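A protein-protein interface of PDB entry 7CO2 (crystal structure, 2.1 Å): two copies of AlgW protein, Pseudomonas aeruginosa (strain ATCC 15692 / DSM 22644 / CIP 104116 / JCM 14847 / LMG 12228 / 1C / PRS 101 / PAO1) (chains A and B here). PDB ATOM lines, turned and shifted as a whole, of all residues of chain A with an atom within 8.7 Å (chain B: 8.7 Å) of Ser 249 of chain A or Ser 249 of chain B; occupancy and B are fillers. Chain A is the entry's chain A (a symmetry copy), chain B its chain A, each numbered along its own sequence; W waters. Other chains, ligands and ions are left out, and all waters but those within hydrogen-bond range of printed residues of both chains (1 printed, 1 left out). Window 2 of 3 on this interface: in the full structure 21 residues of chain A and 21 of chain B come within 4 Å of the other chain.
Of the 14 printed residues of chain A, 6 touch a printed residue of chain B. Printed residues of chain A that touch a printed residue of chain B: Phe 188, Asn 223, Ser 249, Gly 250, Gly 251 and Ser 252. Along chain A the printed residues that touch a printed residue of chain B span positions 188 to 252. Among the printed residues, no Asp or Glu carboxylate lies within 4 Å of a Lys or Arg side-chain nitrogen of the other chain.
Water W1 lies within hydrogen-bond range of the side-chain hydroxyl (OG) of Ser 249 of chain B (2.8 Å), the side-chain hydroxyl (OG) of Ser 249 of chain A (2.8 Å), the side-chain amide nitrogen (NE2) of Gln 253 of chain B (3.3 Å) and the side-chain amide nitrogen (NE2) of Gln 253 of chain A (3.3 Å).
Phe 188 of chain A touches Lys 248 of chain B, but with the chains exchanged Lys 248 of chain A does not touch Phe 188 of chain B (14.1 Å). Ser 249 of chain B touches its own counterpart, Ser 249 of chain A. Gly 250 of chain A touches Lys 248 of chain B, but with the chains exchanged Lys 248 of chain A does not touch Gly 250 of chain B (10.3 Å). Ser 252 of chain A touches Gln 253 of chain B, but with the chains exchanged Gln 253 of chain A does not touch Ser 252 of chain B (6.0 Å). Positions printed for both chains: 188, 223, 224, 245, 246, 247, 248, 249, 250, 251, 252, 253, 254 and 389.
The side-chain hydroxyl (OG) of Ser 249 of chain B sits at hydrogen-bond distance from the backbone carbonyl oxygen (O) of Gly 251 of chain B (3.5 Å). The backbone carbonyl oxygen (O) of Pro 224 of chain A is in hydrogen-bond range of the backbone NH (N) of Phe 188 of chain A (2.7 Å). The side-chain hydroxyl of Ser 247 of chain A lies within hydrogen-bond range of the backbone NH of Ser 249 of chain A, at 2.9 Å. O of Gly 251 of chain A sits at hydrogen-bond distance from OG of Ser 247 of chain A (2.6 Å). O of Gly 251 of chain A sits at hydrogen-bond distance from OG of Ser 249 of chain A. The side-chain hydroxyl (OG) of Ser 252 of chain A is in hydrogen-bond range of the backbone NH (N) of Gly 254 of chain A.
Among the printed residues, merely in contact across the chains: Phe 188 of chain A with Phe 246 of chain B (3.3 Å), Gly 251 of chain A with Gln 253 of chain B (3.4 Å), Phe 188 of chain A with Lys 248 of chain B (3.5 Å), Ser 249 of chain A with Ser 249 of chain B (3.5 Å), Gly 250 of chain A with Lys 248 of chain B (3.7 Å), Ser 252 of chain A with Gln 253 of chain B (3.7 Å), Ser 249 of chain A with Lys 248 of chain B (3.8 Å) and Phe 188 of chain A with Gln 253 of chain B (3.9 Å).
Of chain B, only Lys 248 (3.8 Å), Ser 249 (3.5 Å) and Gln 253 (3.1 Å) come within 4 Å of Ser 249 of chain A. Of the printed residues of chain A, Ser 249 of chain B touches Ser 249. Of the printed residues of chain B, Gly 250 of chain A touches Lys 248 (3.7 Å). Of chain B, only Gln 253 comes within 4 Å of Gly 251 of chain A. No residue of chain A comes within 4 Å of Gly 250 of chain B. No residue of chain A comes within 4 Å of Gly 251 of chain B. Printed residues of chain B within 4 Å of Phe 188 of chain A: Phe 246 (3.3 Å), Lys 248 (3.5 Å) and Gln 253 (3.9 Å). Of the printed residues of chain B, Ser 252 of chain A touches Gln 253. The nearest residue of chain B that does not touch Ser 249 of chain A is Ser 252 of chain B (6.6 Å). The nearest residue of chain A that does not touch Ser 249 of chain B is Gln 253 of chain A (5.6 Å). The nearest printed residue of chain B that does not touch Phe 188 of chain A is Ser 247 of chain B (5.1 Å).
The backbone carbonyl oxygen of Gln 253 of chain B is in hydrogen-bond range of the side-chain amide nitrogen of Asn 223 of chain A, 2.8 Å away. The side-chain hydroxyl (OG) of Ser 249 of chain A is in hydrogen-bond range of the side-chain amide nitrogen (NE2) of Gln 253 of chain B, 3.1 Å away.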
ATOM      1  N   PHE A 188     -16.430  26.148  20.622  1.00  0.00           N
ATOM      2  CA  PHE A 188     -16.770  25.988  22.033  1.00  0.00           C
ATOM      3  C   PHE A 188     -15.671  25.318  22.862  1.00  0.00           C
ATOM      4  O   PHE A 188     -15.977  24.709  23.891  1.00  0.00           O
ATOM      5  CB  PHE A 188     -18.064  25.186  22.201  1.00  0.00           C
ATOM      6  CG  PHE A 188     -19.214  25.775  21.476  1.00  0.00           C
ATOM      7  CD1 PHE A 188     -19.521  27.122  21.641  1.00  0.00           C
ATOM      8  CD2 PHE A 188     -19.949  25.009  20.579  1.00  0.00           C
ATOM      9  CE1 PHE A 188     -20.555  27.694  20.953  1.00  0.00           C
ATOM     10  CE2 PHE A 188     -20.991  25.577  19.893  1.00  0.00           C
ATOM     11  CZ  PHE A 188     -21.288  26.924  20.087  1.00  0.00           C
ATOM     12  N   ASN A 223     -18.474  28.104  14.560  1.00  0.00           N
ATOM     13  CA  ASN A 223     -19.058  28.448  15.847  1.00  0.00           C
ATOM     14  C   ASN A 223     -18.041  29.263  16.610  1.00  0.00           C
ATOM     15  O   ASN A 223     -16.849  29.228  16.286  1.00  0.00           O
ATOM     16  CB  ASN A 223     -19.396  27.212  16.681  1.00  0.00           C
ATOM     17  CG  ASN A 223     -20.677  26.519  16.254  1.00  0.00           C
ATOM     18  OD1 ASN A 223     -21.773  27.028  16.505  1.00  0.00           O
ATOM     19  ND2 ASN A 223     -20.546  25.288  15.731  1.00  0.00           N
ATOM     20  N   PRO A 224     -18.467  29.958  17.661  1.00  0.00           N
ATOM     21  CA  PRO A 224     -17.506  30.598  18.576  1.00  0.00           C
ATOM     22  C   PRO A 224     -16.436  29.609  19.001  1.00  0.00           C
ATOM     23  O   PRO A 224     -16.743  28.513  19.446  1.00  0.00           O
ATOM     24  CB  PRO A 224     -18.383  31.024  19.755  1.00  0.00           C
ATOM     25  CG  PRO A 224     -19.792  31.307  19.067  1.00  0.00           C
ATOM     26  CD  PRO A 224     -19.881  30.233  18.011  1.00  0.00           C
ATOM     27  N   ILE A 245     -19.559  34.829  11.637  1.00  0.00           N
ATOM     28  CA  ILE A 245     -20.776  34.091  11.318  1.00  0.00           C
ATOM     29  C   ILE A 245     -21.958  35.059  11.401  1.00  0.00           C
ATOM     30  O   ILE A 245     -21.930  36.055  12.132  1.00  0.00           O
ATOM     31  CB  ILE A 245     -21.032  32.874  12.262  1.00  0.00           C
ATOM     32  CG1 ILE A 245     -21.414  33.334  13.647  1.00  0.00           C
ATOM     33  CG2 ILE A 245     -19.838  31.954  12.348  1.00  0.00           C
ATOM     34  CD1 ILE A 245     -22.379  32.359  14.364  1.00  0.00           C
ATOM     35  N   PHE A 246     -23.011  34.756  10.659  1.00  0.00           N
ATOM     36  CA  PHE A 246     -24.292  35.426  10.841  1.00  0.00           C
ATOM     37  C   PHE A 246     -25.250  34.424  11.483  1.00  0.00           C
ATOM     38  O   PHE A 246     -25.432  33.306  10.980  1.00  0.00           O
ATOM     39  CB  PHE A 246     -24.832  35.976   9.517  1.00  0.00           C
ATOM     40  CG  PHE A 246     -25.964  36.922   9.711  1.00  0.00           C
ATOM     41  CD1 PHE A 246     -27.193  36.444  10.189  1.00  0.00           C
ATOM     42  CD2 PHE A 246     -25.809  38.295   9.513  1.00  0.00           C
ATOM     43  CE1 PHE A 246     -28.270  37.312  10.438  1.00  0.00           C
ATOM     44  CE2 PHE A 246     -26.891  39.184   9.756  1.00  0.00           C
ATOM     45  CZ  PHE A 246     -28.123  38.676  10.217  1.00  0.00           C
ATOM     46  N   SER A 247     -25.858  34.811  12.598  1.00  0.00           N
ATOM     47  CA  SER A 247     -26.653  33.850  13.342  1.00  0.00           C
ATOM     48  C   SER A 247     -27.659  34.562  14.231  1.00  0.00           C
ATOM     49  O   SER A 247     -27.341  35.565  14.869  1.00  0.00           O
ATOM     50  CB  SER A 247     -25.729  32.948  14.180  1.00  0.00           C
ATOM     51  OG  SER A 247     -26.449  32.212  15.162  1.00  0.00           O
ATOM     52  N   LYS A 248     -28.860  34.001  14.310  1.00  0.00           N
ATOM     53  CA  LYS A 248     -29.834  34.452  15.302  1.00  0.00           C
ATOM     54  C   LYS A 248     -29.633  33.815  16.681  1.00  0.00           C
ATOM     55  O   LYS A 248     -30.233  34.282  17.650  1.00  0.00           O
ATOM     56  CB  LYS A 248     -31.260  34.154  14.838  1.00  0.00           C
ATOM     57  CG  LYS A 248     -31.478  34.266  13.332  1.00  0.00           C
ATOM     58  CD  LYS A 248     -32.379  35.432  12.988  1.00  0.00           C
ATOM     59  CE  LYS A 248     -31.625  36.734  13.131  1.00  0.00           C
ATOM     60  NZ  LYS A 248     -32.309  37.829  12.371  1.00  0.00           N
ATOM     61  N   SER A 249     -28.814  32.770  16.806  1.00  0.00           N
ATOM     62  CA  SER A 249     -28.757  32.007  18.051  1.00  0.00           C
ATOM     63  C   SER A 249     -27.382  31.950  18.722  1.00  0.00           C
ATOM     64  O   SER A 249     -27.195  31.146  19.640  1.00  0.00           O
ATOM     65  CB  SER A 249     -29.223  30.586  17.771  1.00  0.00           C
ATOM     66  OG  SER A 249     -28.335  30.001  16.852  1.00  0.00           O
ATOM     67  N   GLY A 250     -26.411  32.758  18.305  1.00  0.00           N
ATOM     68  CA  GLY A 250     -25.129  32.629  18.949  1.00  0.00           C
ATOM     69  C   GLY A 250     -24.349  31.382  18.583  1.00  0.00           C
ATOM     70  O   GLY A 250     -23.316  31.118  19.202  1.00  0.00           O
ATOM     71  N   GLY A 251     -24.807  30.606  17.594  1.00  0.00           N
ATOM     72  CA  GLY A 251     -24.058  29.485  17.073  1.00  0.00           C
ATOM     73  C   GLY A 251     -24.457  29.245  15.641  1.00  0.00           C
ATOM     74  O   GLY A 251     -25.338  29.911  15.111  1.00  0.00           O
ATOM     75  N   SER A 252     -23.829  28.249  15.024  1.00  0.00           N
ATOM     76  CA  SER A 252     -23.906  28.111  13.573  1.00  0.00           C
ATOM     77  C   SER A 252     -25.332  27.916  13.081  1.00  0.00           C
ATOM     78  O   SER A 252     -26.062  27.055  13.570  1.00  0.00           O
ATOM     79  CB  SER A 252     -23.047  26.936  13.143  1.00  0.00           C
ATOM     80  OG  SER A 252     -23.061  26.782  11.747  1.00  0.00           O
ATOM     81  N   GLN A 253     -25.719  28.708  12.074  1.00  0.00           N
ATOM     82  CA  GLN A 253     -26.916  28.440  11.292  1.00  0.00           C
ATOM     83  C   GLN A 253     -26.593  28.385   9.804  1.00  0.00           C
ATOM     84  O   GLN A 253     -27.451  28.705   8.967  1.00  0.00           O
ATOM     85  CB  GLN A 253     -27.990  29.483  11.590  1.00  0.00           C
ATOM     86  CG  GLN A 253     -28.397  29.384  13.059  1.00  0.00           C
ATOM     87  CD  GLN A 253     -29.352  30.462  13.477  1.00  0.00           C
ATOM     88  OE1 GLN A 253     -29.446  31.509  12.842  1.00  0.00           O
ATOM     89  NE2 GLN A 253     -30.126  30.181  14.511  1.00  0.00           N
ATOM     90  N   GLY A 254     -25.375  27.954   9.464  1.00  0.00           N
ATOM     91  CA  GLY A 254     -25.013  27.706   8.093  1.00  0.00           C
ATOM     92  C   GLY A 254     -24.475  28.888   7.299  1.00  0.00           C
ATOM     93  O   GLY A 254     -24.207  28.731   6.093  1.00  0.00           O
ATOM     94  N   GLU A 389     -23.011  38.240  13.868  1.00  0.00           N
ATOM     95  CA  GLU A 389     -23.653  39.062  12.838  1.00  0.00           C
ATOM     96  C   GLU A 389     -22.746  40.107  12.158  1.00  0.00           C
ATOM     97  O   GLU A 389     -22.995  40.509  11.016  1.00  0.00           O
ATOM     98  CB  GLU A 389     -24.862  39.762  13.439  1.00  0.00           C
ATOM     99  CG  GLU A 389     -26.093  38.875  13.567  1.00  0.00           C
ATOM    100  CD  GLU A 389     -27.299  39.672  14.045  1.00  0.00           C
ATOM    101  OE1 GLU A 389     -28.374  39.077  14.263  1.00  0.00           O
ATOM    102  OE2 GLU A 389     -27.159  40.904  14.207  1.00  0.00           O
ATOM    103  N   PHE B 188     -37.140  16.229  16.642  1.00  0.00           N
ATOM    104  CA  PHE B 188     -38.396  16.923  16.913  1.00  0.00           C
ATOM    105  C   PHE B 188     -39.643  16.105  16.563  1.00  0.00           C
ATOM    106  O   PHE B 188     -40.692  16.692  16.291  1.00  0.00           O
ATOM    107  CB  PHE B 188     -38.462  18.257  16.161  1.00  0.00           C
ATOM    108  CG  PHE B 188     -37.323  19.153  16.464  1.00  0.00           C
ATOM    109  CD1 PHE B 188     -36.987  19.423  17.787  1.00  0.00           C
ATOM    110  CD2 PHE B 188     -36.545  19.676  15.438  1.00  0.00           C
ATOM    111  CE1 PHE B 188     -35.915  20.219  18.089  1.00  0.00           C
ATOM    112  CE2 PHE B 188     -35.477  20.480  15.735  1.00  0.00           C
ATOM    113  CZ  PHE B 188     -35.169  20.748  17.067  1.00  0.00           C
ATOM    114  N   ASN B 223     -30.460  16.570  16.577  1.00  0.00           N
ATOM    115  CA  ASN B 223     -31.385  17.442  17.282  1.00  0.00           C
ATOM    116  C   ASN B 223     -32.097  16.611  18.323  1.00  0.00           C
ATOM    117  O   ASN B 223     -32.118  15.379  18.226  1.00  0.00           O
ATOM    118  CB  ASN B 223     -32.440  18.043  16.353  1.00  0.00           C
ATOM    119  CG  ASN B 223     -31.931  19.209  15.523  1.00  0.00           C
ATOM    120  OD1 ASN B 223     -31.725  20.305  16.052  1.00  0.00           O
ATOM    121  ND2 ASN B 223     -31.860  19.011  14.196  1.00  0.00           N
ATOM    122  N   PRO B 224     -32.742  17.253  19.293  1.00  0.00           N
ATOM    123  CA  PRO B 224     -33.633  16.524  20.212  1.00  0.00           C
ATOM    124  C   PRO B 224     -34.597  15.648  19.436  1.00  0.00           C
ATOM    125  O   PRO B 224     -35.261  16.113  18.520  1.00  0.00           O
ATOM    126  CB  PRO B 224     -34.359  17.648  20.954  1.00  0.00           C
ATOM    127  CG  PRO B 224     -33.281  18.821  20.968  1.00  0.00           C
ATOM    128  CD  PRO B 224     -32.615  18.695  19.620  1.00  0.00           C
ATOM    129  N   ILE B 245     -25.452  16.537  22.043  1.00  0.00           N
ATOM    130  CA  ILE B 245     -25.071  17.669  21.206  1.00  0.00           C
ATOM    131  C   ILE B 245     -24.550  18.783  22.116  1.00  0.00           C
ATOM    132  O   ILE B 245     -24.925  18.890  23.289  1.00  0.00           O
ATOM    133  CB  ILE B 245     -26.243  18.217  20.331  1.00  0.00           C
ATOM    134  CG1 ILE B 245     -27.275  18.913  21.183  1.00  0.00           C
ATOM    135  CG2 ILE B 245     -26.908  17.132  19.518  1.00  0.00           C
ATOM    136  CD1 ILE B 245     -27.983  20.077  20.445  1.00  0.00           C
ATOM    137  N   PHE B 246     -23.692  19.628  21.568  1.00  0.00           N
ATOM    138  CA  PHE B 246     -23.326  20.877  22.223  1.00  0.00           C
ATOM    139  C   PHE B 246     -23.976  22.016  21.438  1.00  0.00           C
ATOM    140  O   PHE B 246     -23.808  22.122  20.213  1.00  0.00           O
ATOM    141  CB  PHE B 246     -21.806  21.035  22.323  1.00  0.00           C
ATOM    142  CG  PHE B 246     -21.406  22.131  23.247  1.00  0.00           C
ATOM    143  CD1 PHE B 246     -21.675  23.463  22.903  1.00  0.00           C
ATOM    144  CD2 PHE B 246     -20.846  21.861  24.498  1.00  0.00           C
ATOM    145  CE1 PHE B 246     -21.363  24.521  23.772  1.00  0.00           C
ATOM    146  CE2 PHE B 246     -20.521  22.922  25.385  1.00  0.00           C
ATOM    147  CZ  PHE B 246     -20.783  24.256  25.006  1.00  0.00           C
ATOM    148  N   SER B 247     -24.724  22.866  22.129  1.00  0.00           N
ATOM    149  CA  SER B 247     -25.496  23.872  21.420  1.00  0.00           C
ATOM    150  C   SER B 247     -25.837  25.032  22.340  1.00  0.00           C
ATOM    151  O   SER B 247     -26.198  24.835  23.500  1.00  0.00           O
ATOM    152  CB  SER B 247     -26.776  23.236  20.848  1.00  0.00           C
ATOM    153  OG  SER B 247     -27.717  24.218  20.428  1.00  0.00           O
ATOM    154  N   LYS B 248     -25.772  26.240  21.795  1.00  0.00           N
ATOM    155  CA  LYS B 248     -26.296  27.409  22.499  1.00  0.00           C
ATOM    156  C   LYS B 248     -27.806  27.597  22.322  1.00  0.00           C
ATOM    157  O   LYS B 248     -28.399  28.399  23.046  1.00  0.00           O
ATOM    158  CB  LYS B 248     -25.595  28.685  22.029  1.00  0.00           C
ATOM    159  CG  LYS B 248     -24.123  28.509  21.667  1.00  0.00           C
ATOM    160  CD  LYS B 248     -23.222  29.234  22.642  1.00  0.00           C
ATOM    161  CE  LYS B 248     -23.149  28.475  23.948  1.00  0.00           C
ATOM    162  NZ  LYS B 248     -21.944  28.887  24.735  1.00  0.00           N
ATOM    163  N   SER B 249     -28.449  26.890  21.392  1.00  0.00           N
ATOM    164  CA  SER B 249     -29.838  27.189  21.051  1.00  0.00           C
ATOM    165  C   SER B 249     -30.824  26.033  21.245  1.00  0.00           C
ATOM    166  O   SER B 249     -31.958  26.126  20.767  1.00  0.00           O
ATOM    167  CB  SER B 249     -29.894  27.641  19.599  1.00  0.00           C
ATOM    168  OG  SER B 249     -29.457  26.580  18.787  1.00  0.00           O
ATOM    169  N   GLY B 250     -30.444  24.949  21.914  1.00  0.00           N
ATOM    170  CA  GLY B 250     -31.404  23.879  22.028  1.00  0.00           C
ATOM    171  C   GLY B 250     -31.646  23.098  20.753  1.00  0.00           C
ATOM    172  O   GLY B 250     -32.559  22.269  20.724  1.00  0.00           O
ATOM    173  N   GLY B 251     -30.857  23.329  19.697  1.00  0.00           N
ATOM    174  CA  GLY B 251     -30.913  22.530  18.494  1.00  0.00           C
ATOM    175  C   GLY B 251     -29.570  22.565  17.813  1.00  0.00           C
ATOM    176  O   GLY B 251     -28.655  23.250  18.257  1.00  0.00           O
ATOM    177  N   SER B 252     -29.468  21.854  16.695  1.00  0.00           N
ATOM    178  CA  SER B 252     -28.160  21.568  16.116  1.00  0.00           C
ATOM    179  C   SER B 252     -27.402  22.831  15.736  1.00  0.00           C
ATOM    180  O   SER B 252     -27.925  23.704  15.045  1.00  0.00           O
ATOM    181  CB  SER B 252     -28.342  20.690  14.892  1.00  0.00           C
ATOM    182  OG  SER B 252     -27.106  20.358  14.317  1.00  0.00           O
ATOM    183  N   GLN B 253     -26.138  22.911  16.168  1.00  0.00           N
ATOM    184  CA  GLN B 253     -25.195  23.882  15.637  1.00  0.00           C
ATOM    185  C   GLN B 253     -23.930  23.196  15.137  1.00  0.00           C
ATOM    186  O   GLN B 253     -22.844  23.797  15.159  1.00  0.00           O
ATOM    187  CB  GLN B 253     -24.876  24.941  16.688  1.00  0.00           C
ATOM    188  CG  GLN B 253     -26.150  25.712  17.033  1.00  0.00           C
ATOM    189  CD  GLN B 253     -25.960  26.685  18.157  1.00  0.00           C
ATOM    190  OE1 GLN B 253     -25.034  26.563  18.956  1.00  0.00           O
ATOM    191  NE2 GLN B 253     -26.795  27.709  18.185  1.00  0.00           N
ATOM    192  N   GLY B 254     -24.061  21.956  14.660  1.00  0.00           N
ATOM    193  CA  GLY B 254     -22.972  21.272  14.014  1.00  0.00           C
ATOM    194  C   GLY B 254     -22.022  20.491  14.910  1.00  0.00           C
ATOM    195  O   GLY B 254     -21.031  19.935  14.398  1.00  0.00           O
ATOM    196  N   GLU B 389     -25.575  20.262  25.868  1.00  0.00           N
ATOM    197  CA  GLU B 389     -24.216  20.580  26.314  1.00  0.00           C
ATOM    198  C   GLU B 389     -23.507  19.478  27.126  1.00  0.00           C
ATOM    199  O   GLU B 389     -22.272  19.411  27.150  1.00  0.00           O
ATOM    200  CB  GLU B 389     -24.244  21.864  27.128  1.00  0.00           C
ATOM    201  CG  GLU B 389     -24.316  23.131  26.286  1.00  0.00           C
ATOM    202  CD  GLU B 389     -24.202  24.377  27.154  1.00  0.00           C
ATOM    203  OE1 GLU B 389     -24.308  25.501  26.623  1.00  0.00           O
ATOM    204  OE2 GLU B 389     -24.011  24.219  28.381  1.00  0.00           O
HETATM  205  O   HOH W   1     -29.292  27.442  16.090  1.00  0.00           O
